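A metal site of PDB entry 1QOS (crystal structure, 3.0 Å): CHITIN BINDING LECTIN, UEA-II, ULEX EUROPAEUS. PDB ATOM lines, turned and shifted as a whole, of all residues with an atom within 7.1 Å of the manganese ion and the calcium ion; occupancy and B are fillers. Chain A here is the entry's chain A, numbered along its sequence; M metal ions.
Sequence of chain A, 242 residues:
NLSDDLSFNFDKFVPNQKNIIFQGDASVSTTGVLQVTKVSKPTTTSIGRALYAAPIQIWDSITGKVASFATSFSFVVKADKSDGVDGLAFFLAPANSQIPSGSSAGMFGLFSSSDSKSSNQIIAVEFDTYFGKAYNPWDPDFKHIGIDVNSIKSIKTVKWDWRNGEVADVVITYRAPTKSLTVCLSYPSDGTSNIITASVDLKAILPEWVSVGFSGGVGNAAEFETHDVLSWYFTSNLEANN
OD1 of Asp 139 sits close to NE1 of Trp 138, 3.4 Å away.
OE2 of Glu 126 lies close to OG of Ser 154, 3.0 Å away.
The side-chain carboxylate (OE1) of Glu 126 lies close to the side-chain carboxylate (OD2) of Asp 148 (2.6 Å).
The backbone carbonyl oxygen (O) of Gly 146 is in hydrogen-bond range of the backbone NH (N) of Glu 126, 2.8 Å away.
ND1 of His 144 sits at hydrogen-bond distance from O of Phe 142, at 2.8 Å.
O of Asp 86 lies within hydrogen-bond range of N of Tyr 130 (3.4 Å).
The backbone carbonyl oxygen (O) of Gly 132 is in hydrogen-bond range of the side-chain hydroxyl (OH) of Tyr 130, 3.2 Å away.
OG of Ser 154 is in hydrogen-bond range of OD1 of Asp 148.
OG of Ser 154 touches the manganese ion, 3.8 Å away.
Five residues have an atom within 4 Å of the manganese ion: Glu 126, Asp 128, Asp 139, His 144 and Ser 154.
Four residues have an atom within 4 Å of the calcium ion: Asp 128, Tyr 130, Asn 136 and Asp 139.
OD1 of Asp 139 is bound to the manganese ion, 1.9 Å away.
The manganese ion is bound by OE2 of Glu 126, 1.9 Å away.
OD2 of Asp 128 is bound to the manganese ion, 2.1 Å away.
A ring nitrogen (NE2) of His 144 binds the manganese ion (2.2 Å).
The manganese ion has four donor atoms within binding distance.
The calcium ion is bound by OD1 of Asp 128 (2.1 Å), OD1 of Asn 136 (2.2 Å), OD2 of Asp 139 (2.3 Å) and O of Tyr 130 (2.4 Å).
The calcium ion has four donor atoms within binding distance.
Slightly farther from the calcium ion lies the side-chain carboxylate (OD2) of Asp 128 (2.9 Å).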
ATOM      1  N   ASP A  86       6.411  18.350  11.919  1.00  0.00           N
ATOM      2  CA  ASP A  86       5.568  17.608  12.853  1.00  0.00           C
ATOM      3  C   ASP A  86       6.338  17.091  14.049  1.00  0.00           C
ATOM      4  O   ASP A  86       5.741  16.763  15.088  1.00  0.00           O
ATOM      5  CB  ASP A  86       4.951  16.391  12.161  1.00  0.00           C
ATOM      6  CG  ASP A  86       3.588  16.666  11.602  1.00  0.00           C
ATOM      7  OD1 ASP A  86       2.625  16.748  12.393  1.00  0.00           O
ATOM      8  OD2 ASP A  86       3.485  16.808  10.365  1.00  0.00           O
ATOM      9  N   GLY A  87       7.646  16.938  13.865  1.00  0.00           N
ATOM     10  CA  GLY A  87       8.491  16.425  14.922  1.00  0.00           C
ATOM     11  C   GLY A  87       9.661  15.605  14.440  1.00  0.00           C
ATOM     12  O   GLY A  87       9.792  15.256  13.264  1.00  0.00           O
ATOM     13  N   ALA A 105       3.482  12.041   8.291  1.00  0.00           N
ATOM     14  CA  ALA A 105       4.332  12.894   9.096  1.00  0.00           C
ATOM     15  C   ALA A 105       4.085  12.728  10.608  1.00  0.00           C
ATOM     16  O   ALA A 105       5.038  12.694  11.389  1.00  0.00           O
ATOM     17  CB  ALA A 105       4.134  14.320   8.698  1.00  0.00           C
ATOM     18  N   GLY A 106       2.826  12.592  11.012  1.00  0.00           N
ATOM     19  CA  GLY A 106       2.516  12.428  12.421  1.00  0.00           C
ATOM     20  C   GLY A 106       2.991  11.119  13.013  1.00  0.00           C
ATOM     21  O   GLY A 106       2.976  10.950  14.235  1.00  0.00           O
ATOM     22  N   MET A 107       3.381  10.175  12.158  1.00  0.00           N
ATOM     23  CA  MET A 107       3.861   8.861  12.615  1.00  0.00           C
ATOM     24  C   MET A 107       5.371   8.740  12.359  1.00  0.00           C
ATOM     25  O   MET A 107       5.955   7.648  12.398  1.00  0.00           O
ATOM     26  CB  MET A 107       3.053   7.736  11.950  1.00  0.00           C
ATOM     27  CG  MET A 107       1.538   7.865  12.173  1.00  0.00           C
ATOM     28  SD  MET A 107       0.476   6.584  11.452  1.00  0.00           S
ATOM     29  CE  MET A 107       0.776   6.806   9.667  1.00  0.00           C
ATOM     30  N   PHE A 108       5.986   9.888  12.102  1.00  0.00           N
ATOM     31  CA  PHE A 108       7.420  10.035  11.850  1.00  0.00           C
ATOM     32  C   PHE A 108       8.050   8.986  10.956  1.00  0.00           C
ATOM     33  O   PHE A 108       9.246   8.734  11.064  1.00  0.00           O
ATOM     34  CB  PHE A 108       8.157  10.126  13.174  1.00  0.00           C
ATOM     35  CG  PHE A 108       7.522  11.055  14.149  1.00  0.00           C
ATOM     36  CD1 PHE A 108       7.547  12.430  13.950  1.00  0.00           C
ATOM     37  CD2 PHE A 108       6.869  10.568  15.275  1.00  0.00           C
ATOM     38  CE1 PHE A 108       6.944  13.304  14.846  1.00  0.00           C
ATOM     39  CE2 PHE A 108       6.260  11.425  16.181  1.00  0.00           C
ATOM     40  CZ  PHE A 108       6.291  12.803  15.969  1.00  0.00           C
ATOM     41  N   GLU A 126      10.302  10.335  20.642  1.00  0.00           N
ATOM     42  CA  GLU A 126       9.767  11.378  19.789  1.00  0.00           C
ATOM     43  C   GLU A 126       9.861  12.772  20.382  1.00  0.00           C
ATOM     44  O   GLU A 126       9.765  12.961  21.593  1.00  0.00           O
ATOM     45  CB  GLU A 126       8.308  11.086  19.417  1.00  0.00           C
ATOM     46  CG  GLU A 126       7.352  11.047  20.600  1.00  0.00           C
ATOM     47  CD  GLU A 126       5.887  10.975  20.190  1.00  0.00           C
ATOM     48  OE1 GLU A 126       5.555  10.271  19.204  1.00  0.00           O
ATOM     49  OE2 GLU A 126       5.060  11.632  20.854  1.00  0.00           O
ATOM     50  N   PHE A 127      10.057  13.724  19.483  1.00  0.00           N
ATOM     51  CA  PHE A 127      10.138  15.148  19.796  1.00  0.00           C
ATOM     52  C   PHE A 127       9.029  15.762  18.950  1.00  0.00           C
ATOM     53  O   PHE A 127       9.289  16.335  17.903  1.00  0.00           O
ATOM     54  CB  PHE A 127      11.499  15.684  19.424  1.00  0.00           C
ATOM     55  CG  PHE A 127      12.608  15.066  20.198  1.00  0.00           C
ATOM     56  CD1 PHE A 127      12.967  15.570  21.446  1.00  0.00           C
ATOM     57  CD2 PHE A 127      13.281  13.947  19.702  1.00  0.00           C
ATOM     58  CE1 PHE A 127      13.977  14.963  22.199  1.00  0.00           C
ATOM     59  CE2 PHE A 127      14.296  13.342  20.442  1.00  0.00           C
ATOM     60  CZ  PHE A 127      14.643  13.853  21.694  1.00  0.00           C
ATOM     61  N   ASP A 128       7.810  15.525  19.413  1.00  0.00           N
ATOM     62  CA  ASP A 128       6.558  15.954  18.790  1.00  0.00           C
ATOM     63  C   ASP A 128       6.322  17.457  18.874  1.00  0.00           C
ATOM     64  O   ASP A 128       6.204  17.981  19.985  1.00  0.00           O
ATOM     65  CB  ASP A 128       5.416  15.236  19.514  1.00  0.00           C
ATOM     66  CG  ASP A 128       4.407  14.617  18.575  1.00  0.00           C
ATOM     67  OD1 ASP A 128       4.084  15.256  17.560  1.00  0.00           O
ATOM     68  OD2 ASP A 128       3.930  13.490  18.872  1.00  0.00           O
ATOM     69  N   THR A 129       6.234  18.141  17.741  1.00  0.00           N
ATOM     70  CA  THR A 129       5.978  19.589  17.713  1.00  0.00           C
ATOM     71  C   THR A 129       4.501  19.879  17.431  1.00  0.00           C
ATOM     72  O   THR A 129       3.992  20.965  17.732  1.00  0.00           O
ATOM     73  CB  THR A 129       6.788  20.321  16.632  1.00  0.00           C
ATOM     74  OG1 THR A 129       6.652  19.622  15.388  1.00  0.00           O
ATOM     75  CG2 THR A 129       8.235  20.394  17.010  1.00  0.00           C
ATOM     76  N   TYR A 130       3.833  18.908  16.829  1.00  0.00           N
ATOM     77  CA  TYR A 130       2.421  19.025  16.513  1.00  0.00           C
ATOM     78  C   TYR A 130       1.582  18.084  17.370  1.00  0.00           C
ATOM     79  O   TYR A 130       1.791  16.869  17.359  1.00  0.00           O
ATOM     80  CB  TYR A 130       2.174  18.741  15.042  1.00  0.00           C
ATOM     81  CG  TYR A 130       0.718  18.739  14.700  1.00  0.00           C
ATOM     82  CD1 TYR A 130       0.003  19.928  14.582  1.00  0.00           C
ATOM     83  CD2 TYR A 130       0.025  17.544  14.564  1.00  0.00           C
ATOM     84  CE1 TYR A 130      -1.368  19.932  14.347  1.00  0.00           C
ATOM     85  CE2 TYR A 130      -1.343  17.529  14.317  1.00  0.00           C
ATOM     86  CZ  TYR A 130      -2.034  18.721  14.219  1.00  0.00           C
ATOM     87  OH  TYR A 130      -3.403  18.721  14.000  1.00  0.00           O
ATOM     88  N   PHE A 131       0.575  18.640  18.020  1.00  0.00           N
ATOM     89  CA  PHE A 131      -0.286  17.885  18.918  1.00  0.00           C
ATOM     90  C   PHE A 131      -1.778  18.096  18.723  1.00  0.00           C
ATOM     91  O   PHE A 131      -2.579  17.668  19.559  1.00  0.00           O
ATOM     92  CB  PHE A 131       0.071  18.244  20.356  1.00  0.00           C
ATOM     93  CG  PHE A 131      -0.029  19.716  20.642  1.00  0.00           C
ATOM     94  CD1 PHE A 131       0.924  20.603  20.149  1.00  0.00           C
ATOM     95  CD2 PHE A 131      -1.057  20.220  21.422  1.00  0.00           C
ATOM     96  CE1 PHE A 131       0.846  21.971  20.412  1.00  0.00           C
ATOM     97  CE2 PHE A 131      -1.153  21.578  21.699  1.00  0.00           C
ATOM     98  CZ  PHE A 131      -0.196  22.460  21.198  1.00  0.00           C
ATOM     99  N   GLY A 132      -2.149  18.769  17.628  1.00  0.00           N
ATOM    100  CA  GLY A 132      -3.553  19.034  17.326  1.00  0.00           C
ATOM    101  C   GLY A 132      -4.397  17.775  17.238  1.00  0.00           C
ATOM    102  O   GLY A 132      -4.052  16.833  16.530  1.00  0.00           O
ATOM    103  N   ASN A 136      -3.983  14.393  15.100  1.00  0.00           N
ATOM    104  CA  ASN A 136      -3.168  13.615  16.047  1.00  0.00           C
ATOM    105  C   ASN A 136      -3.945  13.499  17.354  1.00  0.00           C
ATOM    106  O   ASN A 136      -3.609  14.143  18.344  1.00  0.00           O
ATOM    107  CB  ASN A 136      -1.836  14.321  16.351  1.00  0.00           C
ATOM    108  CG  ASN A 136      -0.778  14.123  15.281  1.00  0.00           C
ATOM    109  OD1 ASN A 136       0.401  14.361  15.530  1.00  0.00           O
ATOM    110  ND2 ASN A 136      -1.186  13.700  14.085  1.00  0.00           N
ATOM    111  N   TRP A 138      -4.097  11.118  19.590  1.00  0.00           N
ATOM    112  CA  TRP A 138      -3.370  10.435  20.653  1.00  0.00           C
ATOM    113  C   TRP A 138      -2.491  11.350  21.504  1.00  0.00           C
ATOM    114  O   TRP A 138      -2.311  11.097  22.694  1.00  0.00           O
ATOM    115  CB  TRP A 138      -2.490   9.351  20.049  1.00  0.00           C
ATOM    116  CG  TRP A 138      -1.632   9.858  18.938  1.00  0.00           C
ATOM    117  CD1 TRP A 138      -0.482  10.575  19.061  1.00  0.00           C
ATOM    118  CD2 TRP A 138      -1.880   9.741  17.529  1.00  0.00           C
ATOM    119  NE1 TRP A 138       0.007  10.918  17.829  1.00  0.00           N
ATOM    120  CE2 TRP A 138      -0.825  10.414  16.866  1.00  0.00           C
ATOM    121  CE3 TRP A 138      -2.881   9.131  16.765  1.00  0.00           C
ATOM    122  CZ2 TRP A 138      -0.747  10.495  15.462  1.00  0.00           C
ATOM    123  CZ3 TRP A 138      -2.808   9.209  15.374  1.00  0.00           C
ATOM    124  CH2 TRP A 138      -1.741   9.892  14.734  1.00  0.00           C
ATOM    125  N   ASP A 139      -1.943  12.399  20.893  1.00  0.00           N
ATOM    126  CA  ASP A 139      -1.058  13.347  21.570  1.00  0.00           C
ATOM    127  C   ASP A 139      -1.743  14.176  22.657  1.00  0.00           C
ATOM    128  O   ASP A 139      -2.952  14.423  22.598  1.00  0.00           O
ATOM    129  CB  ASP A 139      -0.416  14.311  20.543  1.00  0.00           C
ATOM    130  CG  ASP A 139       0.722  13.669  19.735  1.00  0.00           C
ATOM    131  OD1 ASP A 139       1.424  12.765  20.252  1.00  0.00           O
ATOM    132  OD2 ASP A 139       0.938  14.106  18.586  1.00  0.00           O
ATOM    133  N   PRO A 140      -0.979  14.578  23.675  1.00  0.00           N
ATOM    134  CA  PRO A 140      -1.471  15.420  24.778  1.00  0.00           C
ATOM    135  C   PRO A 140      -1.618  16.868  24.321  1.00  0.00           C
ATOM    136  O   PRO A 140      -1.323  17.204  23.170  1.00  0.00           O
ATOM    137  CB  PRO A 140      -0.364  15.275  25.824  1.00  0.00           C
ATOM    138  CG  PRO A 140       0.848  15.102  25.002  1.00  0.00           C
ATOM    139  CD  PRO A 140       0.391  14.112  23.961  1.00  0.00           C
ATOM    140  N   PHE A 142       0.072  19.572  24.382  1.00  0.00           N
ATOM    141  CA  PHE A 142       1.285  20.390  24.295  1.00  0.00           C
ATOM    142  C   PHE A 142       2.417  19.732  23.520  1.00  0.00           C
ATOM    143  O   PHE A 142       2.376  18.527  23.238  1.00  0.00           O
ATOM    144  CB  PHE A 142       1.774  20.788  25.693  1.00  0.00           C
ATOM    145  CG  PHE A 142       1.776  19.659  26.678  1.00  0.00           C
ATOM    146  CD1 PHE A 142       2.404  18.449  26.381  1.00  0.00           C
ATOM    147  CD2 PHE A 142       1.153  19.797  27.896  1.00  0.00           C
ATOM    148  CE1 PHE A 142       2.393  17.389  27.287  1.00  0.00           C
ATOM    149  CE2 PHE A 142       1.130  18.743  28.806  1.00  0.00           C
ATOM    150  CZ  PHE A 142       1.752  17.543  28.500  1.00  0.00           C
ATOM    151  N   HIS A 144       5.609  17.898  23.090  1.00  0.00           N
ATOM    152  CA  HIS A 144       6.145  16.938  24.028  1.00  0.00           C
ATOM    153  C   HIS A 144       7.325  16.078  23.566  1.00  0.00           C
ATOM    154  O   HIS A 144       7.685  16.043  22.390  1.00  0.00           O
ATOM    155  CB  HIS A 144       5.003  16.002  24.443  1.00  0.00           C
ATOM    156  CG  HIS A 144       4.314  15.336  23.278  1.00  0.00           C
ATOM    157  ND1 HIS A 144       3.370  15.984  22.511  1.00  0.00           N
ATOM    158  CD2 HIS A 144       4.436  14.095  22.752  1.00  0.00           C
ATOM    159  CE1 HIS A 144       2.933  15.170  21.560  1.00  0.00           C
ATOM    160  NE2 HIS A 144       3.560  14.015  21.685  1.00  0.00           N
ATOM    161  N   ILE A 145       7.928  15.414  24.542  1.00  0.00           N
ATOM    162  CA  ILE A 145       8.996  14.439  24.320  1.00  0.00           C
ATOM    163  C   ILE A 145       8.273  13.179  24.739  1.00  0.00           C
ATOM    164  O   ILE A 145       7.609  13.159  25.795  1.00  0.00           O
ATOM    165  CB  ILE A 145      10.179  14.624  25.296  1.00  0.00           C
ATOM    166  CG1 ILE A 145      10.941  15.908  24.989  1.00  0.00           C
ATOM    167  CG2 ILE A 145      11.120  13.446  25.189  1.00  0.00           C
ATOM    168  CD1 ILE A 145      12.126  16.110  25.890  1.00  0.00           C
ATOM    169  N   GLY A 146       8.345  12.134  23.931  1.00  0.00           N
ATOM    170  CA  GLY A 146       7.661  10.916  24.299  1.00  0.00           C
ATOM    171  C   GLY A 146       8.422   9.641  24.010  1.00  0.00           C
ATOM    172  O   GLY A 146       9.247   9.586  23.094  1.00  0.00           O
ATOM    173  N   ASP A 148       8.029   6.030  22.785  1.00  0.00           N
ATOM    174  CA  ASP A 148       7.070   5.261  22.019  1.00  0.00           C
ATOM    175  C   ASP A 148       7.471   3.815  21.949  1.00  0.00           C
ATOM    176  O   ASP A 148       8.605   3.500  21.578  1.00  0.00           O
ATOM    177  CB  ASP A 148       6.948   5.809  20.597  1.00  0.00           C
ATOM    178  CG  ASP A 148       6.480   7.248  20.569  1.00  0.00           C
ATOM    179  OD1 ASP A 148       5.923   7.735  21.572  1.00  0.00           O
ATOM    180  OD2 ASP A 148       6.692   7.900  19.525  1.00  0.00           O
ATOM    181  N   ILE A 152       2.518   4.805  18.221  1.00  0.00           N
ATOM    182  CA  ILE A 152       2.739   6.252  18.190  1.00  0.00           C
ATOM    183  C   ILE A 152       2.109   6.947  19.416  1.00  0.00           C
ATOM    184  O   ILE A 152       2.359   8.139  19.676  1.00  0.00           O
ATOM    185  CB  ILE A 152       2.197   6.850  16.874  1.00  0.00           C
ATOM    186  CG1 ILE A 152       2.673   8.293  16.717  1.00  0.00           C
ATOM    187  CG2 ILE A 152       0.693   6.743  16.830  1.00  0.00           C
ATOM    188  CD1 ILE A 152       4.164   8.443  16.484  1.00  0.00           C
ATOM    189  N   LYS A 153       1.278   6.214  20.158  1.00  0.00           N
ATOM    190  CA  LYS A 153       0.669   6.730  21.376  1.00  0.00           C
ATOM    191  C   LYS A 153       1.696   6.436  22.468  1.00  0.00           C
ATOM    192  O   LYS A 153       1.810   5.312  22.970  1.00  0.00           O
ATOM    193  CB  LYS A 153      -0.669   6.032  21.664  1.00  0.00           C
ATOM    194  CG  LYS A 153      -1.427   6.611  22.857  1.00  0.00           C
ATOM    195  CD  LYS A 153      -2.850   6.078  22.959  1.00  0.00           C
ATOM    196  CE  LYS A 153      -3.544   6.572  24.235  1.00  0.00           C
ATOM    197  NZ  LYS A 153      -3.490   8.070  24.385  1.00  0.00           N
ATOM    198  N   SER A 154       2.506   7.442  22.768  1.00  0.00           N
ATOM    199  CA  SER A 154       3.573   7.345  23.766  1.00  0.00           C
ATOM    200  C   SER A 154       3.084   6.712  25.058  1.00  0.00           C
ATOM    201  O   SER A 154       1.928   6.890  25.425  1.00  0.00           O
ATOM    202  CB  SER A 154       4.150   8.724  24.075  1.00  0.00           C
ATOM    203  OG  SER A 154       4.303   9.501  22.896  1.00  0.00           O
ATOM    204  N   THR A 157       4.949  10.719  28.452  1.00  0.00           N
ATOM    205  CA  THR A 157       5.362  11.968  27.816  1.00  0.00           C
ATOM    206  C   THR A 157       5.682  13.003  28.875  1.00  0.00           C
ATOM    207  O   THR A 157       5.439  12.798  30.058  1.00  0.00           O
ATOM    208  CB  THR A 157       4.247  12.560  26.905  1.00  0.00           C
ATOM    209  OG1 THR A 157       3.021  12.658  27.646  1.00  0.00           O
ATOM    210  CG2 THR A 157       4.028  11.688  25.684  1.00  0.00           C
HETATM  211 MN    MN M   1       3.266  12.233  20.436  1.00  0.00          MN
HETATM  212 CA    CA M   2       2.255  14.623  16.767  1.00  0.00          CA
